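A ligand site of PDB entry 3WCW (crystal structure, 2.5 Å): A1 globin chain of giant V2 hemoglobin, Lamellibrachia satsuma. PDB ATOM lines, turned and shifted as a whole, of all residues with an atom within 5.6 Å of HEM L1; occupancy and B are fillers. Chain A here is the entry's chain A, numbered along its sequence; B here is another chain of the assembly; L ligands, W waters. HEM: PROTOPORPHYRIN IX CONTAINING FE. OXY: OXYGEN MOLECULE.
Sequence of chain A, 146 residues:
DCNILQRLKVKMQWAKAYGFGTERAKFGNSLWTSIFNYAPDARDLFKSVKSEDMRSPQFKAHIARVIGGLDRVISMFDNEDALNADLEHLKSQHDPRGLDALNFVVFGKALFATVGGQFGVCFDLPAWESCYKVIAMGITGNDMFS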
ATOM      1  N   TRP A  32     -36.351  18.096  13.837  1.00  0.00           N
ATOM      2  CA  TRP A  32     -36.039  18.602  12.509  1.00  0.00           C
ATOM      3  C   TRP A  32     -37.091  18.379  11.427  1.00  0.00           C
ATOM      4  O   TRP A  32     -37.178  19.156  10.476  1.00  0.00           O
ATOM      5  CB  TRP A  32     -34.698  18.049  12.084  1.00  0.00           C
ATOM      6  CG  TRP A  32     -33.613  18.764  12.802  1.00  0.00           C
ATOM      7  CD1 TRP A  32     -32.985  18.370  13.940  1.00  0.00           C
ATOM      8  CD2 TRP A  32     -33.080  20.040  12.463  1.00  0.00           C
ATOM      9  NE1 TRP A  32     -32.086  19.323  14.329  1.00  0.00           N
ATOM     10  CE2 TRP A  32     -32.123  20.356  13.435  1.00  0.00           C
ATOM     11  CE3 TRP A  32     -33.315  20.949  11.415  1.00  0.00           C
ATOM     12  CZ2 TRP A  32     -31.386  21.563  13.412  1.00  0.00           C
ATOM     13  CZ3 TRP A  32     -32.590  22.136  11.376  1.00  0.00           C
ATOM     14  CH2 TRP A  32     -31.636  22.433  12.378  1.00  0.00           C
ATOM     15  N   ALA A  42     -36.072  26.700   5.055  1.00  0.00           N
ATOM     16  CA  ALA A  42     -34.928  26.614   5.936  1.00  0.00           C
ATOM     17  C   ALA A  42     -34.035  25.414   5.600  1.00  0.00           C
ATOM     18  O   ALA A  42     -32.852  25.390   5.941  1.00  0.00           O
ATOM     19  CB  ALA A  42     -35.370  26.543   7.396  1.00  0.00           C
ATOM     20  N   LEU A  45     -30.741  25.829   3.737  1.00  0.00           N
ATOM     21  CA  LEU A  45     -29.633  26.398   4.523  1.00  0.00           C
ATOM     22  C   LEU A  45     -28.703  25.305   5.036  1.00  0.00           C
ATOM     23  O   LEU A  45     -27.618  25.597   5.519  1.00  0.00           O
ATOM     24  CB  LEU A  45     -30.147  27.164   5.737  1.00  0.00           C
ATOM     25  CG  LEU A  45     -31.081  28.362   5.511  1.00  0.00           C
ATOM     26  CD1 LEU A  45     -31.812  28.666   6.800  1.00  0.00           C
ATOM     27  CD2 LEU A  45     -30.276  29.546   5.019  1.00  0.00           C
ATOM     28  N   PHE A  46     -29.145  24.058   4.935  1.00  0.00           N
ATOM     29  CA  PHE A  46     -28.365  22.952   5.451  1.00  0.00           C
ATOM     30  C   PHE A  46     -27.790  21.987   4.419  1.00  0.00           C
ATOM     31  O   PHE A  46     -27.701  20.781   4.678  1.00  0.00           O
ATOM     32  CB  PHE A  46     -29.212  22.175   6.452  1.00  0.00           C
ATOM     33  CG  PHE A  46     -29.582  22.983   7.640  1.00  0.00           C
ATOM     34  CD1 PHE A  46     -28.695  23.101   8.706  1.00  0.00           C
ATOM     35  CD2 PHE A  46     -30.800  23.649   7.697  1.00  0.00           C
ATOM     36  CE1 PHE A  46     -29.025  23.866   9.816  1.00  0.00           C
ATOM     37  CE2 PHE A  46     -31.142  24.422   8.791  1.00  0.00           C
ATOM     38  CZ  PHE A  46     -30.256  24.541   9.857  1.00  0.00           C
ATOM     39  N   SER A  48     -24.794  21.822   3.625  1.00  0.00           N
ATOM     40  CA  SER A  48     -23.493  21.409   4.143  1.00  0.00           C
ATOM     41  C   SER A  48     -23.565  20.175   5.047  1.00  0.00           C
ATOM     42  O   SER A  48     -22.535  19.694   5.527  1.00  0.00           O
ATOM     43  CB  SER A  48     -22.842  22.558   4.912  1.00  0.00           C
ATOM     44  OG  SER A  48     -23.690  23.017   5.963  1.00  0.00           O
ATOM     45  N   VAL A  49     -24.771  19.669   5.281  1.00  0.00           N
ATOM     46  CA  VAL A  49     -24.951  18.489   6.125  1.00  0.00           C
ATOM     47  C   VAL A  49     -26.027  17.608   5.488  1.00  0.00           C
ATOM     48  O   VAL A  49     -26.772  16.917   6.176  1.00  0.00           O
ATOM     49  CB  VAL A  49     -25.331  18.861   7.606  1.00  0.00           C
ATOM     50  CG1 VAL A  49     -24.102  19.381   8.353  1.00  0.00           C
ATOM     51  CG2 VAL A  49     -26.429  19.919   7.630  1.00  0.00           C
ATOM     52  N   HIS A  62     -25.523  15.891  12.182  1.00  0.00           N
ATOM     53  CA  HIS A  62     -25.890  17.262  12.492  1.00  0.00           C
ATOM     54  C   HIS A  62     -26.995  17.254  13.548  1.00  0.00           C
ATOM     55  O   HIS A  62     -26.933  18.038  14.494  1.00  0.00           O
ATOM     56  CB  HIS A  62     -26.385  17.984  11.241  1.00  0.00           C
ATOM     57  CG  HIS A  62     -26.940  19.338  11.520  1.00  0.00           C
ATOM     58  ND1 HIS A  62     -26.148  20.398  11.883  1.00  0.00           N
ATOM     59  CD2 HIS A  62     -28.218  19.791  11.538  1.00  0.00           C
ATOM     60  CE1 HIS A  62     -26.916  21.455  12.121  1.00  0.00           C
ATOM     61  NE2 HIS A  62     -28.178  21.115  11.917  1.00  0.00           N
ATOM     62  N   ARG A  65     -25.489  16.680  16.894  1.00  0.00           N
ATOM     63  CA  ARG A  65     -24.732  17.790  17.456  1.00  0.00           C
ATOM     64  C   ARG A  65     -25.647  18.880  17.995  1.00  0.00           C
ATOM     65  O   ARG A  65     -25.399  19.453  19.040  1.00  0.00           O
ATOM     66  CB  ARG A  65     -23.753  18.377  16.418  1.00  0.00           C
ATOM     67  CG  ARG A  65     -22.473  17.523  16.200  1.00  0.00           C
ATOM     68  CD  ARG A  65     -21.412  18.231  15.331  1.00  0.00           C
ATOM     69  NE  ARG A  65     -21.873  18.497  13.972  1.00  0.00           N
ATOM     70  CZ  ARG A  65     -21.810  17.632  12.961  1.00  0.00           C
ATOM     71  NH1 ARG A  65     -21.289  16.420  13.127  1.00  0.00           N
ATOM     72  NH2 ARG A  65     -22.288  17.977  11.774  1.00  0.00           N
ATOM     73  N   VAL A  66     -26.746  19.116  17.283  1.00  0.00           N
ATOM     74  CA  VAL A  66     -27.706  20.128  17.684  1.00  0.00           C
ATOM     75  C   VAL A  66     -28.444  19.780  18.963  1.00  0.00           C
ATOM     76  O   VAL A  66     -28.609  20.635  19.826  1.00  0.00           O
ATOM     77  CB  VAL A  66     -28.749  20.375  16.586  1.00  0.00           C
ATOM     78  CG1 VAL A  66     -29.746  21.429  17.052  1.00  0.00           C
ATOM     79  CG2 VAL A  66     -28.060  20.811  15.290  1.00  0.00           C
ATOM     80  N   GLY A  69     -26.219  19.870  21.882  1.00  0.00           N
ATOM     81  CA  GLY A  69     -26.010  21.258  22.266  1.00  0.00           C
ATOM     82  C   GLY A  69     -27.150  21.760  23.135  1.00  0.00           C
ATOM     83  O   GLY A  69     -26.958  22.537  24.069  1.00  0.00           O
ATOM     84  N   LEU A  70     -28.359  21.325  22.821  1.00  0.00           N
ATOM     85  CA  LEU A  70     -29.521  21.722  23.614  1.00  0.00           C
ATOM     86  C   LEU A  70     -29.363  21.161  25.012  1.00  0.00           C
ATOM     87  O   LEU A  70     -29.668  21.819  26.010  1.00  0.00           O
ATOM     88  CB  LEU A  70     -30.816  21.167  22.995  1.00  0.00           C
ATOM     89  CG  LEU A  70     -31.362  21.983  21.840  1.00  0.00           C
ATOM     90  CD1 LEU A  70     -32.574  21.281  21.219  1.00  0.00           C
ATOM     91  CD2 LEU A  70     -31.730  23.357  22.378  1.00  0.00           C
ATOM     92  N   ARG A  72     -26.430  20.114  26.633  1.00  0.00           N
ATOM     93  CA  ARG A  72     -25.361  20.733  27.433  1.00  0.00           C
ATOM     94  C   ARG A  72     -25.732  22.142  27.883  1.00  0.00           C
ATOM     95  O   ARG A  72     -25.417  22.541  29.003  1.00  0.00           O
ATOM     96  CB  ARG A  72     -24.035  20.742  26.662  1.00  0.00           C
ATOM     97  CG  ARG A  72     -23.931  21.723  25.512  1.00  0.00           C
ATOM     98  CD  ARG A  72     -22.595  21.516  24.825  1.00  0.00           C
ATOM     99  NE  ARG A  72     -22.062  22.773  24.323  1.00  0.00           N
ATOM    100  CZ  ARG A  72     -21.892  23.068  23.044  1.00  0.00           C
ATOM    101  NH1 ARG A  72     -22.210  22.189  22.113  1.00  0.00           N
ATOM    102  NH2 ARG A  72     -21.412  24.252  22.689  1.00  0.00           N
ATOM    103  N   LEU A  90     -21.445  29.088  20.821  1.00  0.00           N
ATOM    104  CA  LEU A  90     -22.399  28.719  19.788  1.00  0.00           C
ATOM    105  C   LEU A  90     -22.663  29.916  18.893  1.00  0.00           C
ATOM    106  O   LEU A  90     -22.838  29.766  17.685  1.00  0.00           O
ATOM    107  CB  LEU A  90     -23.727  28.241  20.404  1.00  0.00           C
ATOM    108  CG  LEU A  90     -23.683  27.064  21.392  1.00  0.00           C
ATOM    109  CD1 LEU A  90     -25.077  26.741  21.934  1.00  0.00           C
ATOM    110  CD2 LEU A  90     -23.104  25.876  20.664  1.00  0.00           C
ATOM    111  N   GLN A  93     -20.265  30.209  16.262  1.00  0.00           N
ATOM    112  CA  GLN A  93     -20.419  29.255  15.184  1.00  0.00           C
ATOM    113  C   GLN A  93     -21.605  29.600  14.291  1.00  0.00           C
ATOM    114  O   GLN A  93     -21.600  29.275  13.109  1.00  0.00           O
ATOM    115  CB  GLN A  93     -20.589  27.828  15.736  1.00  0.00           C
ATOM    116  CG  GLN A  93     -19.348  27.313  16.409  1.00  0.00           C
ATOM    117  CD  GLN A  93     -19.597  26.070  17.248  1.00  0.00           C
ATOM    118  OE1 GLN A  93     -20.465  26.068  18.120  1.00  0.00           O
ATOM    119  NE2 GLN A  93     -18.819  25.022  16.989  1.00  0.00           N
ATOM    120  N   HIS A  94     -22.615  30.277  14.832  1.00  0.00           N
ATOM    121  CA  HIS A  94     -23.751  30.616  13.988  1.00  0.00           C
ATOM    122  C   HIS A  94     -23.630  31.953  13.292  1.00  0.00           C
ATOM    123  O   HIS A  94     -24.189  32.142  12.217  1.00  0.00           O
ATOM    124  CB  HIS A  94     -25.051  30.550  14.794  1.00  0.00           C
ATOM    125  CG  HIS A  94     -25.455  29.158  15.156  1.00  0.00           C
ATOM    126  ND1 HIS A  94     -24.801  28.424  16.121  1.00  0.00           N
ATOM    127  CD2 HIS A  94     -26.432  28.348  14.678  1.00  0.00           C
ATOM    128  CE1 HIS A  94     -25.357  27.235  16.231  1.00  0.00           C
ATOM    129  NE2 HIS A  94     -26.356  27.155  15.363  1.00  0.00           N
ATOM    130  N   ARG A  97     -22.669  32.500   9.512  1.00  0.00           N
ATOM    131  CA  ARG A  97     -23.595  31.984   8.519  1.00  0.00           C
ATOM    132  C   ARG A  97     -24.720  32.940   8.166  1.00  0.00           C
ATOM    133  O   ARG A  97     -25.582  32.596   7.351  1.00  0.00           O
ATOM    134  CB  ARG A  97     -24.131  30.623   8.955  1.00  0.00           C
ATOM    135  CG  ARG A  97     -23.009  29.613   9.060  1.00  0.00           C
ATOM    136  CD  ARG A  97     -23.504  28.206   9.189  1.00  0.00           C
ATOM    137  NE  ARG A  97     -22.483  27.253   8.736  1.00  0.00           N
ATOM    138  CZ  ARG A  97     -21.526  26.736   9.515  1.00  0.00           C
ATOM    139  NH1 ARG A  97     -21.452  27.069  10.800  1.00  0.00           N
ATOM    140  NH2 ARG A  97     -20.650  25.897   9.001  1.00  0.00           N
ATOM    141  N   LEU A  99     -27.505  33.981   9.507  1.00  0.00           N
ATOM    142  CA  LEU A  99     -28.813  33.366   9.611  1.00  0.00           C
ATOM    143  C   LEU A  99     -29.883  34.357  10.049  1.00  0.00           C
ATOM    144  O   LEU A  99     -29.707  35.124  10.996  1.00  0.00           O
ATOM    145  CB  LEU A  99     -28.763  32.199  10.606  1.00  0.00           C
ATOM    146  CG  LEU A  99     -27.735  31.098  10.361  1.00  0.00           C
ATOM    147  CD1 LEU A  99     -27.700  30.173  11.577  1.00  0.00           C
ATOM    148  CD2 LEU A  99     -28.078  30.320   9.100  1.00  0.00           C
ATOM    149  N   ASN A 103     -35.725  32.202  11.942  1.00  0.00           N
ATOM    150  CA  ASN A 103     -35.584  30.744  11.964  1.00  0.00           C
ATOM    151  C   ASN A 103     -35.392  30.194  13.374  1.00  0.00           C
ATOM    152  O   ASN A 103     -35.773  29.059  13.661  1.00  0.00           O
ATOM    153  CB  ASN A 103     -34.454  30.299  11.049  1.00  0.00           C
ATOM    154  CG  ASN A 103     -34.860  30.331   9.588  1.00  0.00           C
ATOM    155  OD1 ASN A 103     -34.041  30.562   8.711  1.00  0.00           O
ATOM    156  ND2 ASN A 103     -36.138  30.087   9.327  1.00  0.00           N
ATOM    157  N   PHE A 104     -34.779  30.987  14.248  1.00  0.00           N
ATOM    158  CA  PHE A 104     -34.601  30.575  15.621  1.00  0.00           C
ATOM    159  C   PHE A 104     -35.990  30.549  16.277  1.00  0.00           C
ATOM    160  O   PHE A 104     -36.251  29.740  17.170  1.00  0.00           O
ATOM    161  CB  PHE A 104     -33.662  31.529  16.358  1.00  0.00           C
ATOM    162  CG  PHE A 104     -32.218  31.275  16.059  1.00  0.00           C
ATOM    163  CD1 PHE A 104     -31.479  30.403  16.842  1.00  0.00           C
ATOM    164  CD2 PHE A 104     -31.623  31.818  14.916  1.00  0.00           C
ATOM    165  CE1 PHE A 104     -30.170  30.054  16.502  1.00  0.00           C
ATOM    166  CE2 PHE A 104     -30.320  31.488  14.567  1.00  0.00           C
ATOM    167  CZ  PHE A 104     -29.589  30.596  15.358  1.00  0.00           C
ATOM    168  N   PHE A 107     -37.429  27.358  15.126  1.00  0.00           N
ATOM    169  CA  PHE A 107     -36.777  26.303  15.901  1.00  0.00           C
ATOM    170  C   PHE A 107     -37.500  26.120  17.244  1.00  0.00           C
ATOM    171  O   PHE A 107     -37.864  25.000  17.618  1.00  0.00           O
ATOM    172  CB  PHE A 107     -35.321  26.681  16.142  1.00  0.00           C
ATOM    173  CG  PHE A 107     -34.496  25.581  16.749  1.00  0.00           C
ATOM    174  CD1 PHE A 107     -34.555  25.313  18.104  1.00  0.00           C
ATOM    175  CD2 PHE A 107     -33.630  24.836  15.957  1.00  0.00           C
ATOM    176  CE1 PHE A 107     -33.779  24.310  18.678  1.00  0.00           C
ATOM    177  CE2 PHE A 107     -32.838  23.833  16.519  1.00  0.00           C
ATOM    178  CZ  PHE A 107     -32.913  23.565  17.887  1.00  0.00           C
ATOM    179  N   TYR A 132     -36.343  29.279  26.371  1.00  0.00           N
ATOM    180  CA  TYR A 132     -35.796  29.128  25.036  1.00  0.00           C
ATOM    181  C   TYR A 132     -35.329  30.486  24.577  1.00  0.00           C
ATOM    182  O   TYR A 132     -34.262  30.617  23.959  1.00  0.00           O
ATOM    183  CB  TYR A 132     -36.822  28.590  24.045  1.00  0.00           C
ATOM    184  CG  TYR A 132     -36.276  28.575  22.624  1.00  0.00           C
ATOM    185  CD1 TYR A 132     -36.609  29.579  21.708  1.00  0.00           C
ATOM    186  CD2 TYR A 132     -35.367  27.592  22.222  1.00  0.00           C
ATOM    187  CE1 TYR A 132     -36.039  29.613  20.431  1.00  0.00           C
ATOM    188  CE2 TYR A 132     -34.785  27.617  20.961  1.00  0.00           C
ATOM    189  CZ  TYR A 132     -35.128  28.622  20.065  1.00  0.00           C
ATOM    190  OH  TYR A 132     -34.547  28.627  18.820  1.00  0.00           O
ATOM    191  N   ILE A 135     -31.916  30.985  25.488  1.00  0.00           N
ATOM    192  CA  ILE A 135     -30.953  30.281  24.657  1.00  0.00           C
ATOM    193  C   ILE A 135     -30.712  30.995  23.331  1.00  0.00           C
ATOM    194  O   ILE A 135     -29.560  31.272  22.966  1.00  0.00           O
ATOM    195  CB  ILE A 135     -31.397  28.814  24.396  1.00  0.00           C
ATOM    196  CG1 ILE A 135     -31.279  28.027  25.716  1.00  0.00           C
ATOM    197  CG2 ILE A 135     -30.509  28.173  23.302  1.00  0.00           C
ATOM    198  CD1 ILE A 135     -31.846  26.600  25.687  1.00  0.00           C
ATOM    199  N   ALA A 136     -31.817  31.313  22.642  1.00  0.00           N
ATOM    200  CA  ALA A 136     -31.822  32.014  21.356  1.00  0.00           C
ATOM    201  C   ALA A 136     -31.092  33.339  21.468  1.00  0.00           C
ATOM    202  O   ALA A 136     -30.361  33.748  20.571  1.00  0.00           O
ATOM    203  CB  ALA A 136     -33.268  32.246  20.899  1.00  0.00           C
ATOM    204  N   ILE A 139     -27.341  32.746  21.501  1.00  0.00           N
ATOM    205  CA  ILE A 139     -26.795  32.309  20.238  1.00  0.00           C
ATOM    206  C   ILE A 139     -26.837  33.371  19.157  1.00  0.00           C
ATOM    207  O   ILE A 139     -25.910  33.459  18.359  1.00  0.00           O
ATOM    208  CB  ILE A 139     -27.477  31.004  19.745  1.00  0.00           C
ATOM    209  CG1 ILE A 139     -27.324  29.914  20.807  1.00  0.00           C
ATOM    210  CG2 ILE A 139     -26.838  30.527  18.439  1.00  0.00           C
ATOM    211  CD1 ILE A 139     -27.935  28.587  20.439  1.00  0.00           C
ATOM    212  N   HIS B  94     -16.080  14.836  11.815  1.00  0.00           N
ATOM    213  CA  HIS B  94     -16.337  16.224  12.217  1.00  0.00           C
ATOM    214  C   HIS B  94     -15.454  16.581  13.421  1.00  0.00           C
ATOM    215  O   HIS B  94     -14.758  17.609  13.429  1.00  0.00           O
ATOM    216  CB  HIS B  94     -17.812  16.412  12.608  1.00  0.00           C
ATOM    217  CG  HIS B  94     -18.195  17.840  12.863  1.00  0.00           C
ATOM    218  ND1 HIS B  94     -18.546  18.708  11.845  1.00  0.00           N
ATOM    219  CD2 HIS B  94     -18.243  18.552  14.013  1.00  0.00           C
ATOM    220  CE1 HIS B  94     -18.791  19.892  12.366  1.00  0.00           C
ATOM    221  NE2 HIS B  94     -18.616  19.838  13.677  1.00  0.00           N
ATOM    222  N   GLN B  98     -12.292  19.296  13.935  1.00  0.00           N
ATOM    223  CA  GLN B  98     -12.231  20.277  15.006  1.00  0.00           C
ATOM    224  C   GLN B  98     -10.933  20.191  15.807  1.00  0.00           C
ATOM    225  O   GLN B  98     -10.586  21.121  16.547  1.00  0.00           O
ATOM    226  CB  GLN B  98     -13.425  20.121  15.951  1.00  0.00           C
ATOM    227  CG  GLN B  98     -14.767  20.424  15.282  1.00  0.00           C
ATOM    228  CD  GLN B  98     -15.949  20.188  16.212  1.00  0.00           C
ATOM    229  OE1 GLN B  98     -16.090  19.113  16.777  1.00  0.00           O
ATOM    230  NE2 GLN B  98     -16.804  21.198  16.356  1.00  0.00           N
HETATM  231  CHA HEM L   1     -24.510  24.050  13.493  1.00  0.00           C
HETATM  232  CHB HEM L   1     -26.641  24.122  17.738  1.00  0.00           C
HETATM  233  CHC HEM L   1     -30.279  26.684  15.919  1.00  0.00           C
HETATM  234  CHD HEM L   1     -28.089  26.642  11.651  1.00  0.00           C
HETATM  235  C1A HEM L   1     -24.767  23.826  14.820  1.00  0.00           C
HETATM  236  C2A HEM L   1     -23.924  23.079  15.654  1.00  0.00           C
HETATM  237  C3A HEM L   1     -24.516  23.092  16.868  1.00  0.00           C
HETATM  238  C4A HEM L   1     -25.747  23.870  16.775  1.00  0.00           C
HETATM  239  CMA HEM L   1     -24.011  22.422  18.147  1.00  0.00           C
HETATM  240  CAA HEM L   1     -22.628  22.397  15.272  1.00  0.00           C
HETATM  241  CBA HEM L   1     -21.419  23.234  15.607  1.00  0.00           C
HETATM  242  CGA HEM L   1     -20.102  22.572  15.220  1.00  0.00           C
HETATM  243  O1A HEM L   1     -19.383  23.102  14.337  1.00  0.00           O
HETATM  244  O2A HEM L   1     -19.805  21.547  15.762  1.00  0.00           O
HETATM  245  C1B HEM L   1     -27.843  24.841  17.652  1.00  0.00           C
HETATM  246  C2B HEM L   1     -28.748  25.041  18.766  1.00  0.00           C
HETATM  247  C3B HEM L   1     -29.833  25.807  18.207  1.00  0.00           C
HETATM  248  C4B HEM L   1     -29.484  25.991  16.837  1.00  0.00           C
HETATM  249  CMB HEM L   1     -28.586  24.561  20.169  1.00  0.00           C
HETATM  250  CAB HEM L   1     -30.993  26.233  18.970  1.00  0.00           C
HETATM  251  CBB HEM L   1     -31.008  27.193  19.861  1.00  0.00           C
HETATM  252  C1C HEM L   1     -29.986  26.889  14.590  1.00  0.00           C
HETATM  253  C2C HEM L   1     -30.883  27.630  13.686  1.00  0.00           C
HETATM  254  C3C HEM L   1     -30.273  27.646  12.429  1.00  0.00           C
HETATM  255  C4C HEM L   1     -28.986  26.876  12.643  1.00  0.00           C
HETATM  256  CMC HEM L   1     -32.228  28.262  14.071  1.00  0.00           C
HETATM  257  CAC HEM L   1     -30.741  28.214  11.282  1.00  0.00           C
HETATM  258  CBC HEM L   1     -31.535  27.922  10.309  1.00  0.00           C
HETATM  259  C1D HEM L   1     -26.907  25.935  11.777  1.00  0.00           C
HETATM  260  C2D HEM L   1     -25.953  25.694  10.628  1.00  0.00           C
HETATM  261  C3D HEM L   1     -24.932  24.946  11.185  1.00  0.00           C
HETATM  262  C4D HEM L   1     -25.274  24.756  12.614  1.00  0.00           C
HETATM  263  CMD HEM L   1     -26.164  26.202   9.211  1.00  0.00           C
HETATM  264  CAD HEM L   1     -23.687  24.407  10.504  1.00  0.00           C
HETATM  265  CBD HEM L   1     -23.871  23.038   9.922  1.00  0.00           C
HETATM  266  CGD HEM L   1     -22.648  22.511   9.295  1.00  0.00           C
HETATM  267  O1D HEM L   1     -22.482  22.577   8.049  1.00  0.00           O
HETATM  268  O2D HEM L   1     -21.792  21.990  10.025  1.00  0.00           O
HETATM  269  NA  HEM L   1     -25.895  24.317  15.491  1.00  0.00           N
HETATM  270  NB  HEM L   1     -28.247  25.391  16.507  1.00  0.00           N
HETATM  271  NC  HEM L   1     -28.865  26.457  13.909  1.00  0.00           N
HETATM  272  ND  HEM L   1     -26.458  25.366  12.914  1.00  0.00           N
HETATM  273 FE   HEM L   1     -27.358  25.402  14.695  1.00  0.00          FE
HETATM  274  O1  OXY L   2     -28.206  23.927  14.089  1.00  0.00           O
HETATM  275  O2  OXY L   2     -28.882  23.647  13.087  1.00  0.00           O
HETATM  276  CHA HEM L   3     -12.169  21.057  21.557  1.00  0.00           C
HETATM  277  CHB HEM L   3     -14.028  16.725  22.267  1.00  0.00           C
HETATM  278  CHC HEM L   3      -9.660  14.950  23.326  1.00  0.00           C
HETATM  279  CHD HEM L   3      -7.785  19.318  22.538  1.00  0.00           C
HETATM  280  C1A HEM L   3     -13.085  20.029  21.655  1.00  0.00           C
HETATM  281  C2A HEM L   3     -14.460  20.196  21.439  1.00  0.00           C
HETATM  282  C3A HEM L   3     -15.011  18.972  21.623  1.00  0.00           C
HETATM  283  C4A HEM L   3     -13.936  18.024  21.976  1.00  0.00           C
HETATM  284  CMA HEM L   3     -16.497  18.600  21.506  1.00  0.00           C
HETATM  285  CAA HEM L   3     -15.194  21.472  21.078  1.00  0.00           C
HETATM  286  CBA HEM L   3     -15.511  21.606  19.630  1.00  0.00           C
HETATM  287  CGA HEM L   3     -16.241  22.903  19.290  1.00  0.00           C
HETATM  288  O1A HEM L   3     -15.578  23.901  18.946  1.00  0.00           O
HETATM  289  O2A HEM L   3     -17.425  22.932  19.391  1.00  0.00           O
HETATM  290  C1B HEM L   3     -13.006  15.807  22.632  1.00  0.00           C
HETATM  291  C2B HEM L   3     -13.240  14.407  22.953  1.00  0.00           C
HETATM  292  C3B HEM L   3     -11.926  13.894  23.278  1.00  0.00           C
HETATM  293  C4B HEM L   3     -11.047  15.007  23.114  1.00  0.00           C
HETATM  294  CMB HEM L   3     -14.545  13.685  22.949  1.00  0.00           C
HETATM  295  CAB HEM L   3     -11.686  12.518  23.673  1.00  0.00           C
HETATM  296  CBB HEM L   3     -11.098  11.619  22.918  1.00  0.00           C
HETATM  297  C1C HEM L   3      -8.775  16.005  23.187  1.00  0.00           C
HETATM  298  C2C HEM L   3      -7.326  15.851  23.433  1.00  0.00           C
HETATM  299  C3C HEM L   3      -6.729  17.115  23.210  1.00  0.00           C
HETATM  300  C4C HEM L   3      -7.918  17.998  22.824  1.00  0.00           C
HETATM  301  CMC HEM L   3      -6.635  14.558  23.854  1.00  0.00           C
HETATM  302  CAC HEM L   3      -5.426  17.451  23.319  1.00  0.00           C
HETATM  303  CBC HEM L   3      -4.590  17.840  24.215  1.00  0.00           C
HETATM  304  C1D HEM L   3      -8.824  20.187  22.201  1.00  0.00           C
HETATM  305  C2D HEM L   3      -8.622  21.658  21.901  1.00  0.00           C
HETATM  306  C3D HEM L   3      -9.879  22.125  21.635  1.00  0.00           C
HETATM  307  C4D HEM L   3     -10.808  20.979  21.752  1.00  0.00           C
HETATM  308  CMD HEM L   3      -7.272  22.382  21.933  1.00  0.00           C
HETATM  309  CAD HEM L   3     -10.262  23.550  21.284  1.00  0.00           C
HETATM  310  CBD HEM L   3     -10.531  24.373  22.520  1.00  0.00           C
HETATM  311  CGD HEM L   3     -10.912  25.770  22.220  1.00  0.00           C
HETATM  312  O1D HEM L   3     -12.051  26.026  21.701  1.00  0.00           O
HETATM  313  O2D HEM L   3     -10.091  26.695  22.493  1.00  0.00           O
HETATM  314  NA  HEM L   3     -12.745  18.703  21.982  1.00  0.00           N
HETATM  315  NB  HEM L   3     -11.730  16.182  22.722  1.00  0.00           N
HETATM  316  NC  HEM L   3      -9.081  17.310  22.823  1.00  0.00           N
HETATM  317  ND  HEM L   3     -10.126  19.841  22.092  1.00  0.00           N
HETATM  318 FE   HEM L   3     -10.915  18.006  22.391  1.00  0.00          FE
HETATM  319  O   HOH W   1     -23.230  20.621  12.158  1.00  0.00           O
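An oxygen (O1) of OXY L2 binds an iron atom (FE) of HEM L1.
ND1 of His 94 of chain A is in hydrogen-bond range of O of Leu 90 (2.8 Å).
The guanidinium group (NH1) of Arg 97 is in hydrogen-bond range of the backbone carbonyl oxygen (O) of Gln 93, at 3.2 Å.
O of Phe 104 lies within hydrogen-bond range of OH of Tyr 132 (2.6 Å).
NE2 of His 94 of chain A binds FE of HEM L1 (2.1 Å).
An oxygen (O1D) of HEM L1 is in hydrogen-bond range of the side-chain hydroxyl (OG) of Ser 48, at 2.5 Å.
O2A of HEM L1 lies within hydrogen-bond range of NE2 of His 94 of chain B.
The side-chain amide nitrogen (NE2) of Gln 98 of chain B is in hydrogen-bond range of an oxygen (O2A) of HEM L1, at 3.1 Å.
The side-chain amide nitrogen (NE2) of Gln 93 sits close to an oxygen (O1A) of HEM L1 (3.3 Å).
An oxygen (O1D) of HEM L1 lies within salt-bridge range of the guanidinium group (NH2) of Arg 97 (3.9 Å).
A ring nitrogen (NE2) of His 62 is in hydrogen-bond range of an oxygen (O2) of OXY L2 (2.9 Å).
The side-chain amide nitrogen (NE2) of Gln 93 sits at hydrogen-bond distance from an oxygen (O2A) of HEM L3 (3.5 Å).
Water W1 lies within hydrogen-bond range of the guanidinium group of Arg 65 (2.8 Å), an oxygen (O2D) of HEM L1 (2.9 Å) and a ring nitrogen (ND1) of His 62 (2.9 Å).
Leu 45 touches HEM L1.
CE1 of Phe 46 touches CHD of HEM L1, at 3.5 Å.
CG1 of Val 49 touches CGD of HEM L1 (3.6 Å).
His 62 touches HEM L1 (CE1 to C4D, 3.7 Å).
O of Arg 65 touches CMA of HEM L1 (3.4 Å).
O of Val 66 touches CMB of HEM L1, 3.9 Å away.
Leu 99 touches HEM L1 (CD1 to CHD, 3.6 Å).
Asn 103 touches HEM L1 (O to CMC, 3.7 Å).
Phe 104 touches HEM L1.
Phe 107 touches HEM L1.
Tyr 132 touches HEM L1 (CE2 to CBB, 3.96 Å).
Ile 135 touches HEM L1 (CG2 to CBB, 3.6 Å).
Ile 139 touches HEM L1.
Hydrophobic or aromatic side chains that line HEM L1: Leu 45, Phe 46, Val 49, His 62, Val 66, His 94 of chain A, Leu 99, Phe 104, Phe 107, Tyr 132, Ile 135, Ile 139 and His 94 of chain B.
19 residues have an atom within 4 Å of HEM L1: Leu 45, Phe 46, Ser 48, Val 49, His 62, Arg 65, Val 66, Gln 93, His 94 of chain A, Arg 97, Leu 99, Asn 103, Phe 104, Phe 107, Tyr 132, Ile 135, Ile 139, His 94 of chain B and Gln 98 of chain B.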
